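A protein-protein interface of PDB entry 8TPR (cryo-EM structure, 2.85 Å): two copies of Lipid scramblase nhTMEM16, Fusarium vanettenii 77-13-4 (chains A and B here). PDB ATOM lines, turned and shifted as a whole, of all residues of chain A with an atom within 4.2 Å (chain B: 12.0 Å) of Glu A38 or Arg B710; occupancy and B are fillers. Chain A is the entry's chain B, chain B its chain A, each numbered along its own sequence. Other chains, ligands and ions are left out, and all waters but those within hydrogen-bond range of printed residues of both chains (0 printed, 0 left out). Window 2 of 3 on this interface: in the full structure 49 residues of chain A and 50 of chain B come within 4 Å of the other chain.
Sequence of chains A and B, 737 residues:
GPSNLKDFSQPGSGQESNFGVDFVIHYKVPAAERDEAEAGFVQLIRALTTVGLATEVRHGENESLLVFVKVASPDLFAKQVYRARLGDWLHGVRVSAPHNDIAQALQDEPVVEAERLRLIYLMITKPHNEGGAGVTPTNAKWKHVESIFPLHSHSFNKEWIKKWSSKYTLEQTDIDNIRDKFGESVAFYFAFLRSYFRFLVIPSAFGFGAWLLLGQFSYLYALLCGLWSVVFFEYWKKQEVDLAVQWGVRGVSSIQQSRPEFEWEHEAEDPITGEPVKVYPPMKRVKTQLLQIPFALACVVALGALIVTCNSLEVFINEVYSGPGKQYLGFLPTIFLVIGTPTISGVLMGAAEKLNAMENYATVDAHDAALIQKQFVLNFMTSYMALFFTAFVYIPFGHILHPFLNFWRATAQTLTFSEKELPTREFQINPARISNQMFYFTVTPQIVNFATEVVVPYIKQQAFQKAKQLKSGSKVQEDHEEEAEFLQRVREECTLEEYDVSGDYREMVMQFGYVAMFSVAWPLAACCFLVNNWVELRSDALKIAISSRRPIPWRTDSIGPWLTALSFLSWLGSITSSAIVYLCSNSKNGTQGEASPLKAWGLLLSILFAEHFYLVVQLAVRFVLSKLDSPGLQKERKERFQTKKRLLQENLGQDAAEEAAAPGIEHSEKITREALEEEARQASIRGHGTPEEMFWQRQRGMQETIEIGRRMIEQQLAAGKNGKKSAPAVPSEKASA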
ATOM      1  N   ARG A  34      15.772  19.825   2.649  1.00  0.00           N
ATOM      2  CA  ARG A  34      16.298  20.896   3.489  1.00  0.00           C
ATOM      3  C   ARG A  34      17.527  21.544   2.861  1.00  0.00           C
ATOM      4  O   ARG A  34      17.676  22.772   2.891  1.00  0.00           O
ATOM      5  CB  ARG A  34      16.600  20.363   4.896  1.00  0.00           C
ATOM      6  CG  ARG A  34      17.760  19.377   5.007  1.00  0.00           C
ATOM      7  CD  ARG A  34      19.059  20.071   5.398  1.00  0.00           C
ATOM      8  NE  ARG A  34      19.092  20.429   6.812  1.00  0.00           N
ATOM      9  CZ  ARG A  34      19.465  19.610   7.785  1.00  0.00           C
ATOM     10  NH1 ARG A  34      19.842  18.367   7.535  1.00  0.00           N
ATOM     11  NH2 ARG A  34      19.459  20.049   9.039  1.00  0.00           N
ATOM     12  N   ASP A  35      18.411  20.734   2.269  1.00  0.00           N
ATOM     13  CA  ASP A  35      19.672  21.261   1.754  1.00  0.00           C
ATOM     14  C   ASP A  35      19.427  22.328   0.698  1.00  0.00           C
ATOM     15  O   ASP A  35      19.920  23.458   0.814  1.00  0.00           O
ATOM     16  CB  ASP A  35      20.519  20.124   1.186  1.00  0.00           C
ATOM     17  CG  ASP A  35      21.701  19.782   2.069  1.00  0.00           C
ATOM     18  OD1 ASP A  35      21.617  20.014   3.293  1.00  0.00           O
ATOM     19  OD2 ASP A  35      22.715  19.281   1.538  1.00  0.00           O
ATOM     20  N   GLU A  36      18.632  21.999  -0.323  1.00  0.00           N
ATOM     21  CA  GLU A  36      18.276  22.989  -1.333  1.00  0.00           C
ATOM     22  C   GLU A  36      17.607  24.200  -0.704  1.00  0.00           C
ATOM     23  O   GLU A  36      17.791  25.327  -1.175  1.00  0.00           O
ATOM     24  CB  GLU A  36      17.366  22.357  -2.387  1.00  0.00           C
ATOM     25  CG  GLU A  36      16.734  23.345  -3.355  1.00  0.00           C
ATOM     26  CD  GLU A  36      17.762  24.167  -4.110  1.00  0.00           C
ATOM     27  OE1 GLU A  36      18.820  23.612  -4.474  1.00  0.00           O
ATOM     28  OE2 GLU A  36      17.510  25.369  -4.337  1.00  0.00           O
ATOM     29  N   ALA A  37      16.844  23.991   0.367  1.00  0.00           N
ATOM     30  CA  ALA A  37      16.261  25.119   1.081  1.00  0.00           C
ATOM     31  C   ALA A  37      17.310  25.867   1.891  1.00  0.00           C
ATOM     32  O   ALA A  37      17.311  27.105   1.913  1.00  0.00           O
ATOM     33  CB  ALA A  37      15.130  24.637   1.988  1.00  0.00           C
ATOM     34  N   GLU A  38      18.223  25.137   2.539  1.00  0.00           N
ATOM     35  CA  GLU A  38      19.127  25.761   3.503  1.00  0.00           C
ATOM     36  C   GLU A  38      19.950  26.864   2.852  1.00  0.00           C
ATOM     37  O   GLU A  38      19.939  28.012   3.308  1.00  0.00           O
ATOM     38  CB  GLU A  38      20.037  24.705   4.125  1.00  0.00           C
ATOM     39  CG  GLU A  38      20.896  25.218   5.264  1.00  0.00           C
ATOM     40  CD  GLU A  38      22.370  25.237   4.913  1.00  0.00           C
ATOM     41  OE1 GLU A  38      22.699  25.160   3.711  1.00  0.00           O
ATOM     42  OE2 GLU A  38      23.202  25.320   5.840  1.00  0.00           O
ATOM     43  N   ALA A  39      20.637  26.541   1.756  1.00  0.00           N
ATOM     44  CA  ALA A  39      21.358  27.573   1.019  1.00  0.00           C
ATOM     45  C   ALA A  39      20.402  28.651   0.534  1.00  0.00           C
ATOM     46  O   ALA A  39      20.692  29.848   0.651  1.00  0.00           O
ATOM     47  CB  ALA A  39      22.116  26.953  -0.154  1.00  0.00           C
ATOM     48  N   GLY A  40      19.237  28.243   0.026  1.00  0.00           N
ATOM     49  CA  GLY A  40      18.232  29.211  -0.370  1.00  0.00           C
ATOM     50  C   GLY A  40      17.857  30.150   0.754  1.00  0.00           C
ATOM     51  O   GLY A  40      17.563  31.325   0.513  1.00  0.00           O
ATOM     52  N   PHE A  41      17.888  29.660   1.997  1.00  0.00           N
ATOM     53  CA  PHE A  41      17.621  30.529   3.137  1.00  0.00           C
ATOM     54  C   PHE A  41      18.573  31.715   3.142  1.00  0.00           C
ATOM     55  O   PHE A  41      18.144  32.869   3.256  1.00  0.00           O
ATOM     56  CB  PHE A  41      17.737  29.743   4.441  1.00  0.00           C
ATOM     57  CG  PHE A  41      17.660  30.599   5.670  1.00  0.00           C
ATOM     58  CD1 PHE A  41      16.603  31.474   5.853  1.00  0.00           C
ATOM     59  CD2 PHE A  41      18.646  30.536   6.637  1.00  0.00           C
ATOM     60  CE1 PHE A  41      16.532  32.265   6.979  1.00  0.00           C
ATOM     61  CE2 PHE A  41      18.578  31.326   7.764  1.00  0.00           C
ATOM     62  CZ  PHE A  41      17.520  32.190   7.935  1.00  0.00           C
ATOM     63  N   VAL A  42      19.872  31.453   2.987  1.00  0.00           N
ATOM     64  CA  VAL A  42      20.823  32.556   2.918  1.00  0.00           C
ATOM     65  C   VAL A  42      20.533  33.406   1.689  1.00  0.00           C
ATOM     66  O   VAL A  42      20.605  34.641   1.741  1.00  0.00           O
ATOM     67  CB  VAL A  42      22.274  32.028   2.949  1.00  0.00           C
ATOM     68  CG1 VAL A  42      22.419  30.930   3.991  1.00  0.00           C
ATOM     69  CG2 VAL A  42      22.736  31.546   1.580  1.00  0.00           C
ATOM     70  N   GLN B 699      20.614  39.588  17.138  1.00  0.00           N
ATOM     71  CA  GLN B 699      21.452  39.277  15.975  1.00  0.00           C
ATOM     72  C   GLN B 699      21.406  40.494  15.051  1.00  0.00           C
ATOM     73  O   GLN B 699      20.534  40.602  14.186  1.00  0.00           O
ATOM     74  CB  GLN B 699      20.970  38.011  15.281  1.00  0.00           C
ATOM     75  CG  GLN B 699      19.462  37.896  15.249  1.00  0.00           C
ATOM     76  CD  GLN B 699      18.969  36.494  14.975  1.00  0.00           C
ATOM     77  OE1 GLN B 699      19.223  35.577  15.752  1.00  0.00           O
ATOM     78  NE2 GLN B 699      18.283  36.313  13.856  1.00  0.00           N
ATOM     79  N   MET B 702      25.436  40.580   9.918  1.00  0.00           N
ATOM     80  CA  MET B 702      25.151  39.848   8.690  1.00  0.00           C
ATOM     81  C   MET B 702      25.417  38.355   8.847  1.00  0.00           C
ATOM     82  O   MET B 702      24.517  37.534   8.651  1.00  0.00           O
ATOM     83  CB  MET B 702      25.996  40.432   7.549  1.00  0.00           C
ATOM     84  CG  MET B 702      25.467  40.200   6.141  1.00  0.00           C
ATOM     85  SD  MET B 702      23.673  40.145   6.021  1.00  0.00           S
ATOM     86  CE  MET B 702      23.416  38.381   5.928  1.00  0.00           C
ATOM     87  N   GLN B 703      26.647  37.989   9.214  1.00  0.00           N
ATOM     88  CA  GLN B 703      27.008  36.579   9.304  1.00  0.00           C
ATOM     89  C   GLN B 703      26.299  35.881  10.458  1.00  0.00           C
ATOM     90  O   GLN B 703      25.989  34.688  10.356  1.00  0.00           O
ATOM     91  CB  GLN B 703      28.521  36.433   9.450  1.00  0.00           C
ATOM     92  CG  GLN B 703      29.047  35.052   9.101  1.00  0.00           C
ATOM     93  CD  GLN B 703      28.509  34.542   7.780  1.00  0.00           C
ATOM     94  OE1 GLN B 703      27.878  33.486   7.720  1.00  0.00           O
ATOM     95  NE2 GLN B 703      28.754  35.291   6.713  1.00  0.00           N
ATOM     96  N   GLU B 704      26.049  36.592  11.561  1.00  0.00           N
ATOM     97  CA  GLU B 704      25.431  35.950  12.716  1.00  0.00           C
ATOM     98  C   GLU B 704      24.007  35.503  12.420  1.00  0.00           C
ATOM     99  O   GLU B 704      23.582  34.451  12.904  1.00  0.00           O
ATOM    100  CB  GLU B 704      25.456  36.882  13.928  1.00  0.00           C
ATOM    101  CG  GLU B 704      24.973  38.296  13.666  1.00  0.00           C
ATOM    102  CD  GLU B 704      25.013  39.153  14.917  1.00  0.00           C
ATOM    103  OE1 GLU B 704      25.262  38.600  16.009  1.00  0.00           O
ATOM    104  OE2 GLU B 704      24.792  40.377  14.814  1.00  0.00           O
ATOM    105  N   THR B 705      23.258  36.279  11.633  1.00  0.00           N
ATOM    106  CA  THR B 705      21.913  35.859  11.254  1.00  0.00           C
ATOM    107  C   THR B 705      21.953  34.556  10.468  1.00  0.00           C
ATOM    108  O   THR B 705      21.165  33.638  10.724  1.00  0.00           O
ATOM    109  CB  THR B 705      21.226  36.958  10.442  1.00  0.00           C
ATOM    110  OG1 THR B 705      20.878  38.047  11.305  1.00  0.00           O
ATOM    111  CG2 THR B 705      19.966  36.426   9.778  1.00  0.00           C
ATOM    112  N   ILE B 706      22.884  34.448   9.517  1.00  0.00           N
ATOM    113  CA  ILE B 706      23.007  33.227   8.725  1.00  0.00           C
ATOM    114  C   ILE B 706      23.416  32.054   9.604  1.00  0.00           C
ATOM    115  O   ILE B 706      22.886  30.946   9.467  1.00  0.00           O
ATOM    116  CB  ILE B 706      24.004  33.434   7.572  1.00  0.00           C
ATOM    117  CG1 ILE B 706      23.730  34.759   6.862  1.00  0.00           C
ATOM    118  CG2 ILE B 706      23.938  32.262   6.602  1.00  0.00           C
ATOM    119  CD1 ILE B 706      22.665  34.669   5.802  1.00  0.00           C
ATOM    120  N   GLU B 707      24.376  32.271  10.503  1.00  0.00           N
ATOM    121  CA  GLU B 707      24.828  31.188  11.370  1.00  0.00           C
ATOM    122  C   GLU B 707      23.686  30.703  12.252  1.00  0.00           C
ATOM    123  O   GLU B 707      23.470  29.494  12.404  1.00  0.00           O
ATOM    124  CB  GLU B 707      26.035  31.664  12.193  1.00  0.00           C
ATOM    125  CG  GLU B 707      26.728  30.660  13.155  1.00  0.00           C
ATOM    126  CD  GLU B 707      25.867  30.029  14.251  1.00  0.00           C
ATOM    127  OE1 GLU B 707      24.724  30.503  14.426  1.00  0.00           O
ATOM    128  OE2 GLU B 707      26.264  29.012  14.857  1.00  0.00           O
ATOM    129  N   ILE B 708      22.935  31.637  12.837  1.00  0.00           N
ATOM    130  CA  ILE B 708      21.844  31.258  13.726  1.00  0.00           C
ATOM    131  C   ILE B 708      20.736  30.567  12.945  1.00  0.00           C
ATOM    132  O   ILE B 708      20.121  29.612  13.431  1.00  0.00           O
ATOM    133  CB  ILE B 708      21.332  32.485  14.500  1.00  0.00           C
ATOM    134  CG1 ILE B 708      22.373  32.917  15.537  1.00  0.00           C
ATOM    135  CG2 ILE B 708      19.990  32.195  15.156  1.00  0.00           C
ATOM    136  CD1 ILE B 708      21.837  33.812  16.632  1.00  0.00           C
ATOM    137  N   GLY B 709      20.474  31.018  11.717  1.00  0.00           N
ATOM    138  CA  GLY B 709      19.505  30.330  10.882  1.00  0.00           C
ATOM    139  C   GLY B 709      19.931  28.913  10.548  1.00  0.00           C
ATOM    140  O   GLY B 709      19.111  27.993  10.547  1.00  0.00           O
ATOM    141  N   ARG B 710      21.219  28.718  10.263  1.00  0.00           N
ATOM    142  CA  ARG B 710      21.722  27.373  10.002  1.00  0.00           C
ATOM    143  C   ARG B 710      21.596  26.490  11.236  1.00  0.00           C
ATOM    144  O   ARG B 710      21.230  25.314  11.132  1.00  0.00           O
ATOM    145  CB  ARG B 710      23.176  27.439   9.532  1.00  0.00           C
ATOM    146  CG  ARG B 710      23.340  27.901   8.092  1.00  0.00           C
ATOM    147  CD  ARG B 710      24.663  27.432   7.510  1.00  0.00           C
ATOM    148  NE  ARG B 710      24.779  27.754   6.093  1.00  0.00           N
ATOM    149  CZ  ARG B 710      25.516  28.742   5.606  1.00  0.00           C
ATOM    150  NH1 ARG B 710      26.225  29.530   6.398  1.00  0.00           N
ATOM    151  NH2 ARG B 710      25.546  28.942   4.292  1.00  0.00           N
ATOM    152  N   ARG B 711      21.891  27.041  12.414  1.00  0.00           N
ATOM    153  CA  ARG B 711      21.737  26.272  13.648  1.00  0.00           C
ATOM    154  C   ARG B 711      20.278  25.911  13.902  1.00  0.00           C
ATOM    155  O   ARG B 711      19.969  24.809  14.365  1.00  0.00           O
ATOM    156  CB  ARG B 711      22.311  27.059  14.829  1.00  0.00           C
ATOM    157  CG  ARG B 711      23.828  27.145  14.843  1.00  0.00           C
ATOM    158  CD  ARG B 711      24.461  25.904  15.452  1.00  0.00           C
ATOM    159  NE  ARG B 711      24.539  24.800  14.504  1.00  0.00           N
ATOM    160  CZ  ARG B 711      25.431  24.710  13.527  1.00  0.00           C
ATOM    161  NH1 ARG B 711      26.345  25.647  13.336  1.00  0.00           N
ATOM    162  NH2 ARG B 711      25.406  23.651  12.722  1.00  0.00           N
ATOM    163  N   MET B 712      19.373  26.838  13.615  1.00  0.00           N
ATOM    164  CA  MET B 712      17.943  26.630  13.771  1.00  0.00           C
ATOM    165  C   MET B 712      17.451  25.551  12.805  1.00  0.00           C
ATOM    166  O   MET B 712      16.564  24.754  13.138  1.00  0.00           O
ATOM    167  CB  MET B 712      17.308  27.988  13.492  1.00  0.00           C
ATOM    168  CG  MET B 712      17.199  28.891  14.718  1.00  0.00           C
ATOM    169  SD  MET B 712      15.687  29.837  14.824  1.00  0.00           S
ATOM    170  CE  MET B 712      14.759  28.660  15.709  1.00  0.00           C
ATOM    171  N   ILE B 713      18.023  25.523  11.598  1.00  0.00           N
ATOM    172  CA  ILE B 713      17.734  24.451  10.646  1.00  0.00           C
ATOM    173  C   ILE B 713      18.230  23.117  11.183  1.00  0.00           C
ATOM    174  O   ILE B 713      17.521  22.105  11.129  1.00  0.00           O
ATOM    175  CB  ILE B 713      18.356  24.775   9.274  1.00  0.00           C
ATOM    176  CG1 ILE B 713      17.376  25.577   8.420  1.00  0.00           C
ATOM    177  CG2 ILE B 713      18.760  23.496   8.545  1.00  0.00           C
ATOM    178  CD1 ILE B 713      16.253  24.751   7.872  1.00  0.00           C
ATOM    179  N   GLU B 714      19.455  23.094  11.715  1.00  0.00           N
ATOM    180  CA  GLU B 714      20.026  21.849  12.223  1.00  0.00           C
ATOM    181  C   GLU B 714      19.215  21.309  13.393  1.00  0.00           C
ATOM    182  O   GLU B 714      18.993  20.098  13.504  1.00  0.00           O
ATOM    183  CB  GLU B 714      21.483  22.072  12.632  1.00  0.00           C
ATOM    184  CG  GLU B 714      22.217  20.840  13.174  1.00  0.00           C
ATOM    185  CD  GLU B 714      22.240  19.658  12.213  1.00  0.00           C
ATOM    186  OE1 GLU B 714      21.183  19.034  11.983  1.00  0.00           O
ATOM    187  OE2 GLU B 714      23.336  19.330  11.711  1.00  0.00           O
ATOM    188  N   GLN B 715      18.770  22.197  14.286  1.00  0.00           N
ATOM    189  CA  GLN B 715      17.963  21.763  15.421  1.00  0.00           C
ATOM    190  C   GLN B 715      16.622  21.196  14.975  1.00  0.00           C
ATOM    191  O   GLN B 715      16.159  20.192  15.526  1.00  0.00           O
ATOM    192  CB  GLN B 715      17.753  22.923  16.392  1.00  0.00           C
ATOM    193  N   GLN B 716      15.983  21.822  13.992  1.00  0.00           N
ATOM    194  CA  GLN B 716      14.698  21.348  13.489  1.00  0.00           C
ATOM    195  C   GLN B 716      14.720  21.186  11.975  1.00  0.00           C
ATOM    196  O   GLN B 716      14.153  22.001  11.248  1.00  0.00           O
ATOM    197  CB  GLN B 716      13.572  22.303  13.892  1.00  0.00           C
ATOM    198  CG  GLN B 716      13.766  22.958  15.245  1.00  0.00           C
ATOM    199  CD  GLN B 716      12.458  23.406  15.869  1.00  0.00           C
ATOM    200  OE1 GLN B 716      11.593  23.962  15.194  1.00  0.00           O
ATOM    201  NE2 GLN B 716      12.312  23.171  17.170  1.00  0.00           N
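OE1 of Glu B714 lies within salt-bridge range of NH2 of Arg A34 (3.6 Å). The guanidinium group (NE) of Arg B710 is in salt-bridge range of the side-chain carboxylate (OE2) of Glu A38 (2.9 Å).
NH2 of Arg A34 touches O of Ile B713, 3.5 Å away. Phe A41 touches Gly B709. CG2 of Ile B706 touches CG1 of Val A42, at 3.3 Å. Val A42 touches Arg B710 (CG1 to NH2, 3.7 Å).
No residue of chain B comes within 4 Å of Asp A35. No residue of chain B comes within 4 Å of Glu A36. Glu A38 touches one residue of chain B. No residue of chain B comes within 4 Å of Ala A39. No residue of chain B comes within 4 Å of Gly A40. Of the printed residues of chain B, Phe A41 touches Gly B709. Gln B703 touches none of the printed residues of chain A. Printed residues of chain A within 4 Å of Ile B706: Val A42. Of the printed residues of chain A, Gly B709 touches Phe A41 (3.4 Å). Of the printed residues of chain A, Arg B710 touches Glu A38 and Val A42. Of the printed residues of chain A, Ile B713 touches Arg A34. The nearest printed residue of chain A that does not touch Ile B713 is Glu A38 (4.3 Å).
Hydrophobic or aromatic side chains of chain B within 4 Å of the printed part of chain A: Ile B706 and Ile B713.
No position is printed for both chains.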
